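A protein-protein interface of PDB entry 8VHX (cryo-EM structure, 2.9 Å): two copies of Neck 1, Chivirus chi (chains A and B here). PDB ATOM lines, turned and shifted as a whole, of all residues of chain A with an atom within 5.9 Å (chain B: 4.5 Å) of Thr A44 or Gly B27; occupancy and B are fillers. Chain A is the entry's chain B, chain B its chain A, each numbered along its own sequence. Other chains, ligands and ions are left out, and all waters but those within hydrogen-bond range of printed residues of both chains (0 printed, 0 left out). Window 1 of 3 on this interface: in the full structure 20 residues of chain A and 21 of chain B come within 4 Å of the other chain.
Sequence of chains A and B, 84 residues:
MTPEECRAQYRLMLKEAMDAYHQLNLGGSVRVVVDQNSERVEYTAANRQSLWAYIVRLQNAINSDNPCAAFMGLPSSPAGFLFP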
ATOM      1  N   SER A  29     -29.554  -7.999 -36.611  1.00  0.00           N
ATOM      2  CA  SER A  29     -29.755  -6.931 -35.646  1.00  0.00           C
ATOM      3  C   SER A  29     -28.409  -6.439 -35.159  1.00  0.00           C
ATOM      4  O   SER A  29     -27.609  -7.214 -34.629  1.00  0.00           O
ATOM      5  CB  SER A  29     -30.601  -7.404 -34.477  1.00  0.00           C
ATOM      6  OG  SER A  29     -30.616  -6.442 -33.439  1.00  0.00           O
ATOM      7  N   VAL A  30     -28.166  -5.152 -35.341  1.00  0.00           N
ATOM      8  CA  VAL A  30     -26.877  -4.561 -35.028  1.00  0.00           C
ATOM      9  C   VAL A  30     -26.759  -4.410 -33.523  1.00  0.00           C
ATOM     10  O   VAL A  30     -27.516  -3.663 -32.899  1.00  0.00           O
ATOM     11  CB  VAL A  30     -26.713  -3.218 -35.735  1.00  0.00           C
ATOM     12  CG1 VAL A  30     -25.378  -2.664 -35.478  1.00  0.00           C
ATOM     13  CG2 VAL A  30     -26.892  -3.406 -37.180  1.00  0.00           C
ATOM     14  N   ARG A  31     -25.816  -5.133 -32.944  1.00  0.00           N
ATOM     15  CA  ARG A  31     -25.478  -4.981 -31.544  1.00  0.00           C
ATOM     16  C   ARG A  31     -24.302  -4.045 -31.340  1.00  0.00           C
ATOM     17  O   ARG A  31     -24.176  -3.443 -30.272  1.00  0.00           O
ATOM     18  CB  ARG A  31     -25.166  -6.348 -30.947  1.00  0.00           C
ATOM     19  CG  ARG A  31     -25.011  -6.371 -29.458  1.00  0.00           C
ATOM     20  CD  ARG A  31     -24.724  -7.761 -28.960  1.00  0.00           C
ATOM     21  NE  ARG A  31     -23.631  -8.375 -29.699  1.00  0.00           N
ATOM     22  CZ  ARG A  31     -22.349  -8.084 -29.532  1.00  0.00           C
ATOM     23  NH1 ARG A  31     -21.449  -8.702 -30.268  1.00  0.00           N
ATOM     24  NH2 ARG A  31     -21.966  -7.184 -28.637  1.00  0.00           N
ATOM     25  N   GLU A  42     -22.406   0.503 -28.946  1.00  0.00           N
ATOM     26  CA  GLU A  42     -22.822  -0.851 -28.649  1.00  0.00           C
ATOM     27  C   GLU A  42     -24.186  -0.796 -27.996  1.00  0.00           C
ATOM     28  O   GLU A  42     -24.438   0.041 -27.129  1.00  0.00           O
ATOM     29  CB  GLU A  42     -21.831  -1.578 -27.756  1.00  0.00           C
ATOM     30  CG  GLU A  42     -20.410  -1.465 -28.221  1.00  0.00           C
ATOM     31  CD  GLU A  42     -19.522  -2.539 -27.646  1.00  0.00           C
ATOM     32  OE1 GLU A  42     -20.025  -3.370 -26.863  1.00  0.00           O
ATOM     33  OE2 GLU A  42     -18.319  -2.555 -27.981  1.00  0.00           O
ATOM     34  N   TYR A  43     -25.053  -1.694 -28.424  1.00  0.00           N
ATOM     35  CA  TYR A  43     -26.450  -1.687 -28.052  1.00  0.00           C
ATOM     36  C   TYR A  43     -26.766  -2.885 -27.177  1.00  0.00           C
ATOM     37  O   TYR A  43     -26.132  -3.935 -27.277  1.00  0.00           O
ATOM     38  CB  TYR A  43     -27.336  -1.719 -29.285  1.00  0.00           C
ATOM     39  CG  TYR A  43     -27.237  -0.519 -30.177  1.00  0.00           C
ATOM     40  CD1 TYR A  43     -27.695   0.711 -29.764  1.00  0.00           C
ATOM     41  CD2 TYR A  43     -26.716  -0.621 -31.445  1.00  0.00           C
ATOM     42  CE1 TYR A  43     -27.619   1.800 -30.580  1.00  0.00           C
ATOM     43  CE2 TYR A  43     -26.639   0.458 -32.263  1.00  0.00           C
ATOM     44  CZ  TYR A  43     -27.094   1.671 -31.828  1.00  0.00           C
ATOM     45  OH  TYR A  43     -27.025   2.774 -32.638  1.00  0.00           O
ATOM     46  N   THR A  44     -27.747  -2.708 -26.307  1.00  0.00           N
ATOM     47  CA  THR A  44     -28.277  -3.825 -25.548  1.00  0.00           C
ATOM     48  C   THR A  44     -29.057  -4.725 -26.486  1.00  0.00           C
ATOM     49  O   THR A  44     -30.054  -4.305 -27.079  1.00  0.00           O
ATOM     50  CB  THR A  44     -29.158  -3.332 -24.410  1.00  0.00           C
ATOM     51  OG1 THR A  44     -28.405  -2.451 -23.571  1.00  0.00           O
ATOM     52  CG2 THR A  44     -29.661  -4.488 -23.594  1.00  0.00           C
ATOM     53  N   ALA A  45     -28.607  -5.962 -26.607  1.00  0.00           N
ATOM     54  CA  ALA A  45     -29.132  -6.844 -27.627  1.00  0.00           C
ATOM     55  C   ALA A  45     -30.614  -7.084 -27.414  1.00  0.00           C
ATOM     56  O   ALA A  45     -31.090  -7.206 -26.284  1.00  0.00           O
ATOM     57  CB  ALA A  45     -28.372  -8.157 -27.609  1.00  0.00           C
ATOM     58  N   ALA A  46     -31.344  -7.137 -28.517  1.00  0.00           N
ATOM     59  CA  ALA A  46     -32.767  -7.389 -28.461  1.00  0.00           C
ATOM     60  C   ALA A  46     -33.043  -8.839 -28.109  1.00  0.00           C
ATOM     61  O   ALA A  46     -32.255  -9.738 -28.407  1.00  0.00           O
ATOM     62  CB  ALA A  46     -33.407  -7.048 -29.793  1.00  0.00           C
ATOM     63  N   GLN B  23     -36.659   1.703 -27.818  1.00  0.00           N
ATOM     64  CA  GLN B  23     -35.311   1.446 -28.311  1.00  0.00           C
ATOM     65  C   GLN B  23     -34.736   0.167 -27.724  1.00  0.00           C
ATOM     66  O   GLN B  23     -33.922  -0.506 -28.363  1.00  0.00           O
ATOM     67  CB  GLN B  23     -34.410   2.635 -28.001  1.00  0.00           C
ATOM     68  CG  GLN B  23     -34.742   3.897 -28.761  1.00  0.00           C
ATOM     69  CD  GLN B  23     -34.827   3.686 -30.251  1.00  0.00           C
ATOM     70  OE1 GLN B  23     -35.903   3.767 -30.838  1.00  0.00           O
ATOM     71  NE2 GLN B  23     -33.695   3.408 -30.875  1.00  0.00           N
ATOM     72  N   LEU B  24     -35.142  -0.182 -26.508  1.00  0.00           N
ATOM     73  CA  LEU B  24     -34.604  -1.355 -25.835  1.00  0.00           C
ATOM     74  C   LEU B  24     -35.098  -2.639 -26.464  1.00  0.00           C
ATOM     75  O   LEU B  24     -34.312  -3.564 -26.698  1.00  0.00           O
ATOM     76  CB  LEU B  24     -34.995  -1.316 -24.368  1.00  0.00           C
ATOM     77  CG  LEU B  24     -34.541  -2.462 -23.484  1.00  0.00           C
ATOM     78  CD1 LEU B  24     -33.060  -2.558 -23.401  1.00  0.00           C
ATOM     79  CD2 LEU B  24     -35.117  -2.256 -22.137  1.00  0.00           C
ATOM     80  N   ASN B  25     -36.396  -2.727 -26.732  1.00  0.00           N
ATOM     81  CA  ASN B  25     -36.919  -3.946 -27.330  1.00  0.00           C
ATOM     82  C   ASN B  25     -36.453  -4.097 -28.766  1.00  0.00           C
ATOM     83  O   ASN B  25     -36.234  -5.217 -29.236  1.00  0.00           O
ATOM     84  CB  ASN B  25     -38.428  -3.944 -27.240  1.00  0.00           C
ATOM     85  CG  ASN B  25     -38.906  -4.174 -25.846  1.00  0.00           C
ATOM     86  OD1 ASN B  25     -38.912  -5.292 -25.346  1.00  0.00           O
ATOM     87  ND2 ASN B  25     -39.263  -3.101 -25.184  1.00  0.00           N
ATOM     88  N   LEU B  26     -36.292  -2.987 -29.478  1.00  0.00           N
ATOM     89  CA  LEU B  26     -35.750  -3.037 -30.827  1.00  0.00           C
ATOM     90  C   LEU B  26     -34.265  -3.345 -30.862  1.00  0.00           C
ATOM     91  O   LEU B  26     -33.746  -3.674 -31.930  1.00  0.00           O
ATOM     92  CB  LEU B  26     -35.950  -1.715 -31.539  1.00  0.00           C
ATOM     93  CG  LEU B  26     -37.335  -1.121 -31.613  1.00  0.00           C
ATOM     94  CD1 LEU B  26     -37.268   0.128 -32.433  1.00  0.00           C
ATOM     95  CD2 LEU B  26     -38.280  -2.083 -32.173  1.00  0.00           C
ATOM     96  N   GLY B  27     -33.572  -3.230 -29.739  1.00  0.00           N
ATOM     97  CA  GLY B  27     -32.135  -3.373 -29.734  1.00  0.00           C
ATOM     98  C   GLY B  27     -31.380  -2.118 -30.081  1.00  0.00           C
ATOM     99  O   GLY B  27     -30.309  -2.197 -30.687  1.00  0.00           O
ATOM    100  N   GLY B  28     -31.911  -0.961 -29.721  1.00  0.00           N
ATOM    101  CA  GLY B  28     -31.245   0.297 -29.958  1.00  0.00           C
ATOM    102  C   GLY B  28     -30.949   1.047 -28.681  1.00  0.00           C
ATOM    103  O   GLY B  28     -30.769   2.267 -28.705  1.00  0.00           O
ATOM    104  N   SER B  29     -30.903   0.337 -27.560  1.00  0.00           N
ATOM    105  CA  SER B  29     -30.592   0.939 -26.273  1.00  0.00           C
ATOM    106  C   SER B  29     -29.089   0.920 -26.080  1.00  0.00           C
ATOM    107  O   SER B  29     -28.454  -0.133 -26.184  1.00  0.00           O
ATOM    108  CB  SER B  29     -31.280   0.203 -25.132  1.00  0.00           C
ATOM    109  OG  SER B  29     -30.959   0.789 -23.891  1.00  0.00           O
ATOM    110  N   ARG B  31     -25.449   0.941 -24.619  1.00  0.00           N
ATOM    111  CA  ARG B  31     -24.686   0.420 -23.507  1.00  0.00           C
ATOM    112  C   ARG B  31     -23.250   0.893 -23.530  1.00  0.00           C
ATOM    113  O   ARG B  31     -22.605   0.928 -22.485  1.00  0.00           O
ATOM    114  CB  ARG B  31     -24.731  -1.110 -23.526  1.00  0.00           C
ATOM    115  CG  ARG B  31     -24.198  -1.816 -22.310  1.00  0.00           C
ATOM    116  CD  ARG B  31     -24.310  -3.309 -22.489  1.00  0.00           C
ATOM    117  NE  ARG B  31     -23.806  -3.723 -23.795  1.00  0.00           N
ATOM    118  CZ  ARG B  31     -22.522  -3.764 -24.136  1.00  0.00           C
ATOM    119  NH1 ARG B  31     -22.188  -4.146 -25.360  1.00  0.00           N
ATOM    120  NH2 ARG B  31     -21.574  -3.444 -23.261  1.00  0.00           N
ATOM    121  N   ALA B  45     -26.676  -1.797 -18.218  1.00  0.00           N
ATOM    122  CA  ALA B  45     -27.677  -2.235 -19.169  1.00  0.00           C
ATOM    123  C   ALA B  45     -29.074  -2.048 -18.612  1.00  0.00           C
ATOM    124  O   ALA B  45     -29.341  -2.331 -17.441  1.00  0.00           O
ATOM    125  CB  ALA B  45     -27.448  -3.692 -19.530  1.00  0.00           C
ATOM    126  N   ALA B  46     -29.959  -1.554 -19.463  1.00  0.00           N
ATOM    127  CA  ALA B  46     -31.363  -1.435 -19.119  1.00  0.00           C
ATOM    128  C   ALA B  46     -32.020  -2.803 -19.065  1.00  0.00           C
ATOM    129  O   ALA B  46     -31.661  -3.714 -19.814  1.00  0.00           O
ATOM    130  CB  ALA B  46     -32.064  -0.562 -20.138  1.00  0.00           C
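N of Thr A44 sits at hydrogen-bond distance from O of Ser B29, 2.7 Å away. The guanidinium group (NH1) of Arg B31 is in salt-bridge range of the side-chain carboxylate (OE1) of Glu A42 (2.7 Å).
The backbone NH of Gly B28 sits at hydrogen-bond distance from the backbone carbonyl oxygen of Gln B23, 2.5 Å away. N of Ser B29 is in hydrogen-bond range of O of Gln B23 (3.2 Å). The backbone NH (N) of Tyr A43 sits at hydrogen-bond distance from the backbone carbonyl oxygen (O) of Arg A31, at 2.7 Å.
Gly B27 touches Val A30. CB of Tyr A43 touches O of Gly B27 (3.3 Å). CD1 of Tyr A43 touches C of Gly B28, at 3.4 Å. Tyr A43 touches Ser B29. CD1 of Leu B24 touches CG2 of Thr A44 (3.9 Å). O of Thr A44 touches CA of Gly B27, at 3.5 Å. Arg B31 touches Thr A44. Ala A46 touches Asn B25. CB of Ala A46 touches C of Leu B26, at 3.9 Å. CB of Ala A46 touches N of Gly B27, 3.8 Å away.
Of the printed residues of chain B, Thr A44 touches Leu B24 (3.9 Å), Gly B27 (3.5 Å), Ser B29 (2.7 Å) and Arg B31 (3.9 Å). Printed residues of chain A within 4 Å of Gly B27: Val A30, Tyr A43, Thr A44 and Ala A46. Of the printed residues of chain A, Leu B24 touches Thr A44. Of the printed residues of chain B, Tyr A43 touches Gly B27, Gly B28 and Ser B29. The nearest printed residue of chain A that does not touch Ser B29 is Glu A42 (4.1 Å).
Of the 10 printed residues of chain B, 7 touch a printed residue of chain A. Hydrophobic or aromatic side chains of chain B that line the printed part of chain A: Leu B24. Along chain A the printed residues that touch a printed residue of chain B span positions 30 to 46.
4 positions are printed for both chains.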
